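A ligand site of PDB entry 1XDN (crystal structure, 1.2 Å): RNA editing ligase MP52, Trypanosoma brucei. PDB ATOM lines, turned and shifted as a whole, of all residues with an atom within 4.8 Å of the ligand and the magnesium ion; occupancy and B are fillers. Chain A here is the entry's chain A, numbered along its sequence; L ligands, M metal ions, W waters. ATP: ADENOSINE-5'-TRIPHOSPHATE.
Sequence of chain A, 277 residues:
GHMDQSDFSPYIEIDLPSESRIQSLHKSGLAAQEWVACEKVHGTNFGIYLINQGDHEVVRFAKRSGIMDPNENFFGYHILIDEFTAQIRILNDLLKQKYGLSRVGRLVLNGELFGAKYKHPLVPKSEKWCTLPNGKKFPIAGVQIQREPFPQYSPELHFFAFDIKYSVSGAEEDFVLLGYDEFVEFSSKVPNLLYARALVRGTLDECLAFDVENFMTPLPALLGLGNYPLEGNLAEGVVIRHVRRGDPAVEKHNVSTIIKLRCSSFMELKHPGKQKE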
ATOM      1  N   TYR A  11      32.340 -28.316 -16.041  1.00  0.00           N
ATOM      2  CA  TYR A  11      32.178 -27.463 -14.881  1.00  0.00           C
ATOM      3  C   TYR A  11      30.819 -27.834 -14.351  1.00  0.00           C
ATOM      4  O   TYR A  11      30.232 -28.867 -14.746  1.00  0.00           O
ATOM      5  CB  TYR A  11      32.375 -25.975 -15.261  1.00  0.00           C
ATOM      6  CG  TYR A  11      32.555 -25.100 -14.038  1.00  0.00           C
ATOM      7  CD1 TYR A  11      33.699 -25.186 -13.266  1.00  0.00           C
ATOM      8  CD2 TYR A  11      31.553 -24.231 -13.616  1.00  0.00           C
ATOM      9  CE1 TYR A  11      33.844 -24.425 -12.119  1.00  0.00           C
ATOM     10  CE2 TYR A  11      31.698 -23.470 -12.469  1.00  0.00           C
ATOM     11  CZ  TYR A  11      32.832 -23.575 -11.723  1.00  0.00           C
ATOM     12  OH  TYR A  11      32.945 -22.812 -10.594  1.00  0.00           O
ATOM     13  N   ILE A  12      30.358 -27.109 -13.367  1.00  0.00           N
ATOM     14  CA  ILE A  12      29.150 -27.474 -12.661  1.00  0.00           C
ATOM     15  C   ILE A  12      28.023 -26.495 -12.857  1.00  0.00           C
ATOM     16  O   ILE A  12      28.212 -25.340 -13.272  1.00  0.00           O
ATOM     17  CB  ILE A  12      29.449 -27.591 -11.159  1.00  0.00           C
ATOM     18  CG1 ILE A  12      30.007 -26.277 -10.613  1.00  0.00           C
ATOM     19  CG2 ILE A  12      30.399 -28.743 -10.920  1.00  0.00           C
ATOM     20  CD1 ILE A  12      29.935 -26.171  -9.133  1.00  0.00           C
ATOM     21  N   GLU A  13      26.838 -27.005 -12.577  1.00  0.00           N
ATOM     22  CA  GLU A  13      25.716 -26.153 -12.245  1.00  0.00           C
ATOM     23  C   GLU A  13      25.682 -25.912 -10.729  1.00  0.00           C
ATOM     24  O   GLU A  13      26.265 -26.669  -9.959  1.00  0.00           O
ATOM     25  CB  GLU A  13      24.425 -26.734 -12.819  1.00  0.00           C
ATOM     26  CG  GLU A  13      24.464 -26.642 -14.357  1.00  0.00           C
ATOM     27  CD  GLU A  13      23.362 -27.394 -15.071  1.00  0.00           C
ATOM     28  OE1 GLU A  13      22.247 -27.512 -14.514  1.00  0.00           O
ATOM     29  OE2 GLU A  13      23.618 -27.862 -16.218  1.00  0.00           O
ATOM     30  N   ILE A  14      25.025 -24.851 -10.344  1.00  0.00           N
ATOM     31  CA  ILE A  14      25.020 -24.413  -8.966  1.00  0.00           C
ATOM     32  C   ILE A  14      23.596 -24.224  -8.535  1.00  0.00           C
ATOM     33  O   ILE A  14      22.809 -23.598  -9.245  1.00  0.00           O
ATOM     34  CB  ILE A  14      25.835 -23.108  -8.825  1.00  0.00           C
ATOM     35  CG1 ILE A  14      27.293 -23.329  -9.239  1.00  0.00           C
ATOM     36  CG2 ILE A  14      25.784 -22.621  -7.405  1.00  0.00           C
ATOM     37  CD1 ILE A  14      28.130 -22.078  -9.309  1.00  0.00           C
ATOM     38  N   CYS A  38      30.866 -14.038  -4.242  1.00  0.00           N
ATOM     39  CA  CYS A  38      31.448 -13.320  -5.373  1.00  0.00           C
ATOM     40  C   CYS A  38      30.396 -13.126  -6.432  1.00  0.00           C
ATOM     41  O   CYS A  38      29.361 -13.781  -6.439  1.00  0.00           O
ATOM     42  CB  CYS A  38      32.640 -14.096  -5.959  1.00  0.00           C
ATOM     43  SG  CYS A  38      33.971 -14.472  -4.802  1.00  0.00           S
ATOM     44  N   GLU A  39      30.648 -12.221  -7.370  1.00  0.00           N
ATOM     45  CA  GLU A  39      29.658 -11.930  -8.398  1.00  0.00           C
ATOM     46  C   GLU A  39      29.426 -13.132  -9.299  1.00  0.00           C
ATOM     47  O   GLU A  39      30.375 -13.794  -9.718  1.00  0.00           O
ATOM     48  CB  GLU A  39      30.125 -10.719  -9.214  1.00  0.00           C
ATOM     49  CG  GLU A  39      29.154 -10.311 -10.299  1.00  0.00           C
ATOM     50  CD  GLU A  39      29.468  -8.994 -10.973  1.00  0.00           C
ATOM     51  OE1 GLU A  39      30.545  -8.415 -10.720  1.00  0.00           O
ATOM     52  OE2 GLU A  39      28.629  -8.567 -11.808  1.00  0.00           O
ATOM     53  N   LYS A  40      28.155 -13.384  -9.596  1.00  0.00           N
ATOM     54  CA  LYS A  40      27.768 -14.347 -10.622  1.00  0.00           C
ATOM     55  C   LYS A  40      27.612 -13.581 -11.934  1.00  0.00           C
ATOM     56  O   LYS A  40      26.768 -12.688 -12.022  1.00  0.00           O
ATOM     57  CB  LYS A  40      26.482 -15.073 -10.259  1.00  0.00           C
ATOM     58  CG  LYS A  40      26.251 -16.301 -11.111  1.00  0.00           C
ATOM     59  CD  LYS A  40      25.089 -17.137 -10.617  1.00  0.00           C
ATOM     60  CE  LYS A  40      25.001 -18.503 -11.288  1.00  0.00           C
ATOM     61  NZ  LYS A  40      24.679 -18.372 -12.737  1.00  0.00           N
ATOM     62  N   VAL A  41      28.477 -13.885 -12.892  1.00  0.00           N
ATOM     63  CA  VAL A  41      28.523 -13.188 -14.167  1.00  0.00           C
ATOM     64  C   VAL A  41      27.689 -13.923 -15.210  1.00  0.00           C
ATOM     65  O   VAL A  41      27.788 -15.145 -15.358  1.00  0.00           O
ATOM     66  CB  VAL A  41      29.997 -13.006 -14.617  1.00  0.00           C
ATOM     67  CG1 VAL A  41      30.094 -12.412 -16.018  1.00  0.00           C
ATOM     68  CG2 VAL A  41      30.695 -12.097 -13.603  1.00  0.00           C
ATOM     69  N   HIS A  42      26.858 -13.156 -15.924  1.00  0.00           N
ATOM     70  CA  HIS A  42      25.975 -13.687 -16.955  1.00  0.00           C
ATOM     71  C   HIS A  42      26.627 -13.623 -18.324  1.00  0.00           C
ATOM     72  O   HIS A  42      26.483 -12.647 -19.060  1.00  0.00           O
ATOM     73  CB  HIS A  42      24.700 -12.883 -16.958  1.00  0.00           C
ATOM     74  CG  HIS A  42      23.635 -13.406 -17.859  1.00  0.00           C
ATOM     75  ND1 HIS A  42      23.116 -14.656 -17.745  1.00  0.00           N
ATOM     76  CD2 HIS A  42      23.049 -12.856 -18.937  1.00  0.00           C
ATOM     77  CE1 HIS A  42      22.137 -14.798 -18.619  1.00  0.00           C
ATOM     78  NE2 HIS A  42      22.020 -13.689 -19.292  1.00  0.00           N
ATOM     79  N   GLY A  43      27.394 -14.657 -18.623  1.00  0.00           N
ATOM     80  CA  GLY A  43      28.025 -14.833 -19.923  1.00  0.00           C
ATOM     81  C   GLY A  43      27.790 -16.258 -20.366  1.00  0.00           C
ATOM     82  O   GLY A  43      26.668 -16.767 -20.319  1.00  0.00           O
ATOM     83  N   ASN A  45      29.808 -20.274 -20.124  1.00  0.00           N
ATOM     84  CA  ASN A  45      30.847 -21.025 -19.447  1.00  0.00           C
ATOM     85  C   ASN A  45      32.047 -21.248 -20.362  1.00  0.00           C
ATOM     86  O   ASN A  45      31.892 -21.581 -21.546  1.00  0.00           O
ATOM     87  CB  ASN A  45      30.284 -22.370 -18.993  1.00  0.00           C
ATOM     88  CG  ASN A  45      31.215 -23.121 -18.097  1.00  0.00           C
ATOM     89  OD1 ASN A  45      32.003 -23.951 -18.550  1.00  0.00           O
ATOM     90  ND2 ASN A  45      31.178 -22.802 -16.822  1.00  0.00           N
ATOM     91  N   ARG A  64      30.660 -24.976 -22.590  1.00  0.00           N
ATOM     92  CA  ARG A  64      29.957 -25.785 -21.614  1.00  0.00           C
ATOM     93  C   ARG A  64      30.034 -27.264 -21.901  1.00  0.00           C
ATOM     94  O   ARG A  64      30.198 -28.087 -20.983  1.00  0.00           O
ATOM     95  CB  ARG A  64      28.484 -25.344 -21.580  1.00  0.00           C
ATOM     96  CG  ARG A  64      27.501 -26.270 -20.903  1.00  0.00           C
ATOM     97  CD  ARG A  64      27.671 -26.249 -19.436  1.00  0.00           C
ATOM     98  NE  ARG A  64      27.302 -24.948 -18.848  1.00  0.00           N
ATOM     99  CZ  ARG A  64      27.625 -24.577 -17.601  1.00  0.00           C
ATOM    100  NH1 ARG A  64      28.323 -25.391 -16.827  1.00  0.00           N
ATOM    101  NH2 ARG A  64      27.264 -23.378 -17.130  1.00  0.00           N
ATOM    102  N   GLU A 112      33.952 -17.344 -16.920  1.00  0.00           N
ATOM    103  CA  GLU A 112      32.825 -16.925 -17.720  1.00  0.00           C
ATOM    104  C   GLU A 112      33.340 -16.015 -18.847  1.00  0.00           C
ATOM    105  O   GLU A 112      34.004 -15.013 -18.575  1.00  0.00           O
ATOM    106  CB  GLU A 112      31.824 -16.144 -16.860  1.00  0.00           C
ATOM    107  CG  GLU A 112      30.432 -16.081 -17.481  1.00  0.00           C
ATOM    108  CD  GLU A 112      29.595 -17.336 -17.294  1.00  0.00           C
ATOM    109  OE1 GLU A 112      30.120 -18.336 -16.734  1.00  0.00           O
ATOM    110  OE2 GLU A 112      28.407 -17.299 -17.683  1.00  0.00           O
ATOM    111  N   GLN A 146      24.287 -12.928 -24.632  1.00  0.00           N
ATOM    112  CA  GLN A 146      23.020 -12.910 -23.909  1.00  0.00           C
ATOM    113  C   GLN A 146      22.107 -11.804 -24.410  1.00  0.00           C
ATOM    114  O   GLN A 146      22.557 -10.719 -24.781  1.00  0.00           O
ATOM    115  CB  GLN A 146      23.258 -12.713 -22.404  1.00  0.00           C
ATOM    116  CG  GLN A 146      24.083 -13.805 -21.770  1.00  0.00           C
ATOM    117  CD  GLN A 146      23.371 -15.141 -21.748  1.00  0.00           C
ATOM    118  OE1 GLN A 146      22.186 -15.224 -22.033  1.00  0.00           O
ATOM    119  NE2 GLN A 146      24.095 -16.186 -21.390  1.00  0.00           N
ATOM    120  N   PHE A 160      36.057 -13.805 -17.061  1.00  0.00           N
ATOM    121  CA  PHE A 160      35.987 -13.661 -15.603  1.00  0.00           C
ATOM    122  C   PHE A 160      36.349 -15.001 -14.979  1.00  0.00           C
ATOM    123  O   PHE A 160      35.556 -15.952 -15.000  1.00  0.00           O
ATOM    124  CB  PHE A 160      34.567 -13.256 -15.229  1.00  0.00           C
ATOM    125  CG  PHE A 160      34.290 -13.077 -13.773  1.00  0.00           C
ATOM    126  CD1 PHE A 160      34.571 -11.903 -13.121  1.00  0.00           C
ATOM    127  CD2 PHE A 160      33.626 -14.062 -13.076  1.00  0.00           C
ATOM    128  CE1 PHE A 160      34.201 -11.740 -11.766  1.00  0.00           C
ATOM    129  CE2 PHE A 160      33.249 -13.911 -11.770  1.00  0.00           C
ATOM    130  CZ  PHE A 160      33.522 -12.757 -11.123  1.00  0.00           C
ATOM    131  N   PHE A 162      36.881 -17.915 -12.341  1.00  0.00           N
ATOM    132  CA  PHE A 162      36.237 -18.279 -11.084  1.00  0.00           C
ATOM    133  C   PHE A 162      36.703 -19.612 -10.486  1.00  0.00           C
ATOM    134  O   PHE A 162      36.294 -19.940  -9.392  1.00  0.00           O
ATOM    135  CB  PHE A 162      34.706 -18.170 -11.143  1.00  0.00           C
ATOM    136  CG  PHE A 162      34.051 -18.908 -12.288  1.00  0.00           C
ATOM    137  CD1 PHE A 162      33.191 -18.238 -13.145  1.00  0.00           C
ATOM    138  CD2 PHE A 162      34.253 -20.265 -12.506  1.00  0.00           C
ATOM    139  CE1 PHE A 162      32.573 -18.904 -14.185  1.00  0.00           C
ATOM    140  CE2 PHE A 162      33.650 -20.920 -13.560  1.00  0.00           C
ATOM    141  CZ  PHE A 162      32.817 -20.245 -14.394  1.00  0.00           C
ATOM    142  N   ALA A 196      37.098 -13.535  -9.883  1.00  0.00           N
ATOM    143  CA  ALA A 196      36.078 -13.409  -8.849  1.00  0.00           C
ATOM    144  C   ALA A 196      36.707 -13.010  -7.530  1.00  0.00           C
ATOM    145  O   ALA A 196      37.614 -13.675  -7.038  1.00  0.00           O
ATOM    146  CB  ALA A 196      35.352 -14.720  -8.703  1.00  0.00           C
ATOM    147  N   GLU A 236      23.561 -10.311 -12.090  1.00  0.00           N
ATOM    148  CA  GLU A 236      22.738 -11.510 -12.065  1.00  0.00           C
ATOM    149  C   GLU A 236      22.477 -11.981 -10.628  1.00  0.00           C
ATOM    150  O   GLU A 236      21.359 -12.369 -10.285  1.00  0.00           O
ATOM    151  CB  GLU A 236      23.402 -12.616 -12.877  1.00  0.00           C
ATOM    152  CG  GLU A 236      22.717 -13.956 -12.764  1.00  0.00           C
ATOM    153  CD  GLU A 236      23.420 -15.102 -13.432  1.00  0.00           C
ATOM    154  OE1 GLU A 236      24.358 -14.887 -14.218  1.00  0.00           O
ATOM    155  OE2 GLU A 236      23.037 -16.244 -13.129  1.00  0.00           O
ATOM    156  N   VAL A 239      27.580 -16.051  -6.307  1.00  0.00           N
ATOM    157  CA  VAL A 239      27.913 -17.416  -5.964  1.00  0.00           C
ATOM    158  C   VAL A 239      28.577 -17.384  -4.596  1.00  0.00           C
ATOM    159  O   VAL A 239      29.483 -16.567  -4.353  1.00  0.00           O
ATOM    160  CB  VAL A 239      28.853 -18.028  -7.011  1.00  0.00           C
ATOM    161  CG1 VAL A 239      29.393 -19.377  -6.575  1.00  0.00           C
ATOM    162  CG2 VAL A 239      28.111 -18.163  -8.346  1.00  0.00           C
ATOM    163  N   LYS A 260      24.091 -20.493  -5.088  1.00  0.00           N
ATOM    164  CA  LYS A 260      23.892 -19.203  -5.741  1.00  0.00           C
ATOM    165  C   LYS A 260      22.667 -18.509  -5.172  1.00  0.00           C
ATOM    166  O   LYS A 260      21.761 -19.158  -4.636  1.00  0.00           O
ATOM    167  CB  LYS A 260      23.729 -19.375  -7.249  1.00  0.00           C
ATOM    168  CG  LYS A 260      22.384 -19.996  -7.611  1.00  0.00           C
ATOM    169  CD  LYS A 260      22.271 -20.382  -9.063  1.00  0.00           C
ATOM    170  CE  LYS A 260      20.937 -21.021  -9.354  1.00  0.00           C
ATOM    171  NZ  LYS A 260      21.028 -21.919 -10.520  1.00  0.00           N
ATOM    172  N   ARG A 262      20.157 -15.291  -6.855  1.00  0.00           N
ATOM    173  CA  ARG A 262      19.915 -14.396  -7.978  1.00  0.00           C
ATOM    174  C   ARG A 262      18.987 -13.277  -7.577  1.00  0.00           C
ATOM    175  O   ARG A 262      18.127 -13.434  -6.699  1.00  0.00           O
ATOM    176  CB  ARG A 262      19.349 -15.113  -9.183  1.00  0.00           C
ATOM    177  CG  ARG A 262      20.367 -15.955  -9.898  1.00  0.00           C
ATOM    178  CD  ARG A 262      19.761 -16.907 -10.857  1.00  0.00           C
ATOM    179  NE  ARG A 262      20.640 -17.225 -11.970  1.00  0.00           N
ATOM    180  CZ  ARG A 262      20.540 -18.343 -12.677  1.00  0.00           C
ATOM    181  NH1 ARG A 262      19.652 -19.281 -12.349  1.00  0.00           N
ATOM    182  NH2 ARG A 262      21.313 -18.509 -13.724  1.00  0.00           N
HETATM  183  PG  ATP L   1      24.288 -21.026 -18.227  1.00  0.00           P
HETATM  184  O1G ATP L   1      23.966 -19.559 -18.095  1.00  0.00           O
HETATM  185  O2G ATP L   1      23.499 -21.751 -19.288  1.00  0.00           O
HETATM  186  O3G ATP L   1      25.780 -21.312 -18.362  1.00  0.00           O
HETATM  187  PB  ATP L   1      23.371 -20.964 -15.535  1.00  0.00           P
HETATM  188  O1B ATP L   1      21.912 -20.795 -15.546  1.00  0.00           O
HETATM  189  O2B ATP L   1      24.179 -19.739 -15.269  1.00  0.00           O
HETATM  190  O3B ATP L   1      23.862 -21.719 -16.843  1.00  0.00           O
HETATM  191  PA  ATP L   1      23.692 -21.981 -12.861  1.00  0.00           P
HETATM  192  O1A ATP L   1      22.683 -20.981 -12.466  1.00  0.00           O
HETATM  193  O2A ATP L   1      23.629 -23.408 -12.369  1.00  0.00           O
HETATM  194  O3A ATP L   1      23.768 -22.102 -14.468  1.00  0.00           O
HETATM  195  O5' ATP L   1      25.093 -21.330 -12.492  1.00  0.00           O
HETATM  196  C5' ATP L   1      26.318 -21.982 -12.736  1.00  0.00           C
HETATM  197  C4' ATP L   1      27.110 -21.238 -13.783  1.00  0.00           C
HETATM  198  O4' ATP L   1      27.362 -19.904 -13.385  1.00  0.00           O
HETATM  199  C3' ATP L   1      28.512 -21.802 -13.938  1.00  0.00           C
HETATM  200  O3' ATP L   1      28.559 -22.997 -14.678  1.00  0.00           O
HETATM  201  C2' ATP L   1      29.285 -20.650 -14.562  1.00  0.00           C
HETATM  202  O2' ATP L   1      29.294 -20.759 -15.976  1.00  0.00           O
HETATM  203  C1' ATP L   1      28.495 -19.425 -14.115  1.00  0.00           C
HETATM  204  N9  ATP L   1      29.194 -18.499 -13.214  1.00  0.00           N
HETATM  205  C8  ATP L   1      29.164 -17.131 -13.327  1.00  0.00           C
HETATM  206  N7  ATP L   1      29.843 -16.543 -12.337  1.00  0.00           N
HETATM  207  C5  ATP L   1      30.299 -17.568 -11.563  1.00  0.00           C
HETATM  208  C6  ATP L   1      31.069 -17.603 -10.394  1.00  0.00           C
HETATM  209  N6  ATP L   1      31.428 -16.516  -9.709  1.00  0.00           N
HETATM  210  N1  ATP L   1      31.412 -18.823  -9.891  1.00  0.00           N
HETATM  211  C2  ATP L   1      31.006 -19.968 -10.504  1.00  0.00           C
HETATM  212  N3  ATP L   1      30.233 -20.010 -11.607  1.00  0.00           N
HETATM  213  C4  ATP L   1      29.907 -18.792 -12.108  1.00  0.00           C
HETATM  214 MG    MG M   1      24.750 -18.300 -16.627  1.00  0.00          MG
HETATM  215  O   HOH W   1      22.594 -18.400 -20.068  1.00  0.00           O
HETATM  216  O   HOH W   2      21.230 -23.014 -18.768  1.00  0.00           O
HETATM  217  O   HOH W   3      24.724 -24.079 -20.050  1.00  0.00           O
HETATM  218  O   HOH W   4      26.621 -19.045 -16.946  1.00  0.00           O
HETATM  219  O   HOH W   5      27.301 -21.658 -20.413  1.00  0.00           O
HETATM  220  O   HOH W   6      22.975 -17.221 -16.234  1.00  0.00           O
HETATM  221  O   HOH W   7      19.759 -21.676 -14.052  1.00  0.00           O
HETATM  222  O   HOH W   8      32.744 -18.905  -7.334  1.00  0.00           O
HETATM  223  O   HOH W   9      25.086 -16.849 -18.065  1.00  0.00           O
HETATM  224  O   HOH W  10      21.249 -24.652 -12.084  1.00  0.00           O
HETATM  225  O   HOH W  11      25.631 -17.025 -15.166  1.00  0.00           O
HETATM  226  O   HOH W  12      23.611 -20.652 -21.776  1.00  0.00           O
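Merely in contact with the ligand: Phe 162 (3.4 Å), Tyr 11 (3.4 Å), Glu 13 (3.4 Å), Val 239 (3.6 Å) and Phe 160 (3.8 Å).
Of the 21 residues printed, 15 come within 4 Å of the ligand.
O of Glu 112 sits at hydrogen-bond distance from N of Phe 160 (2.8 Å).
OE2 of Glu 112 lies close to N of Gly 43, 3.0 Å away.
The backbone carbonyl oxygen (O) of Ile 14 sits at hydrogen-bond distance from the side-chain amino group (NZ) of Lys 260.
The side-chain carboxylate of Glu 236 lies within salt-bridge range of the side-chain amino group of Lys 40 (2.7 Å).
NE of Arg 262 lies within salt-bridge range of OE2 of Glu 236 (2.8 Å).
N of Cys 38 sits at hydrogen-bond distance from O of Val 239.
The side-chain carboxylate (OE1) of Glu 112 sits at hydrogen-bond distance from an oxygen (O2') of the ligand (2.7 Å).
The side-chain amino group of Lys 260 is in salt-bridge range of an oxygen (O1A) of the ligand (2.7 Å).
The backbone carbonyl oxygen (O) of Ile 12 sits at hydrogen-bond distance from an oxygen (O3') of the ligand, at 2.8 Å.
The guanidinium group (NH2) of Arg 64 lies within salt-bridge range of an oxygen (O3G) of the ligand (2.8 Å).
The backbone NH of Ile 14 sits at hydrogen-bond distance from an oxygen (O2A) of the ligand (2.9 Å).
ND2 of Asn 45 lies within hydrogen-bond range of O2' of the ligand (2.9 Å).
O of Glu 39 sits at hydrogen-bond distance from N6 of the ligand.
NZ of Lys 40 is in salt-bridge range of O1A of the ligand, at 3.3 Å.
An oxygen (O1B) of the ligand lies within salt-bridge range of the guanidinium group of Arg 262 (3.0 Å).
The backbone NH (N) of Val 41 sits at hydrogen-bond distance from a nitrogen (N7) of the ligand, 3.0 Å away.
The magnesium ion is bound by water W4 (2.0 Å).
The magnesium ion is bound by an oxygen (O2B) of the ligand, at 2.1 Å.
Water W9 is bound to the magnesium ion.
The magnesium ion is bound by an oxygen (O1G) of the ligand (2.1 Å).
Water W6 binds the magnesium ion, 2.1 Å away.
Water W11 is bound to the magnesium ion (2.1 Å).
Lys 40 touches the magnesium ion.
Glu 112 touches the magnesium ion (OE2 to MG, 3.9 Å).
Of the 21 residues printed, 2 come within 4 Å of the magnesium ion.
Along chain A the residues within 4 Å of the magnesium ion span positions 40 to 112.
Water W6 lies within hydrogen-bond range of ND1 of His 42, OE2 of Glu 236 and NH2 of Arg 262.
Water W9 lies within hydrogen-bond range of the backbone carbonyl oxygen of Gly 43 (2.8 Å), a ring nitrogen (ND1) of His 42 (3.0 Å) and the side-chain carboxylate of Glu 112 (3.4 Å).
Water W5 bridges O3G of the ligand and N of Asn 45.
Water W10 lies within hydrogen-bond range of O2A of the ligand (2.7 Å), NZ of Lys 260 (3.2 Å) and O of Ile 14 (3.4 Å).
Water W3 lies within hydrogen-bond range of O2G of the ligand (2.7 Å) and NE of Arg 64 (3.0 Å).
Water W7 lies within hydrogen-bond range of O1B of the ligand (2.8 Å) and NH1 of Arg 262 (2.9 Å).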
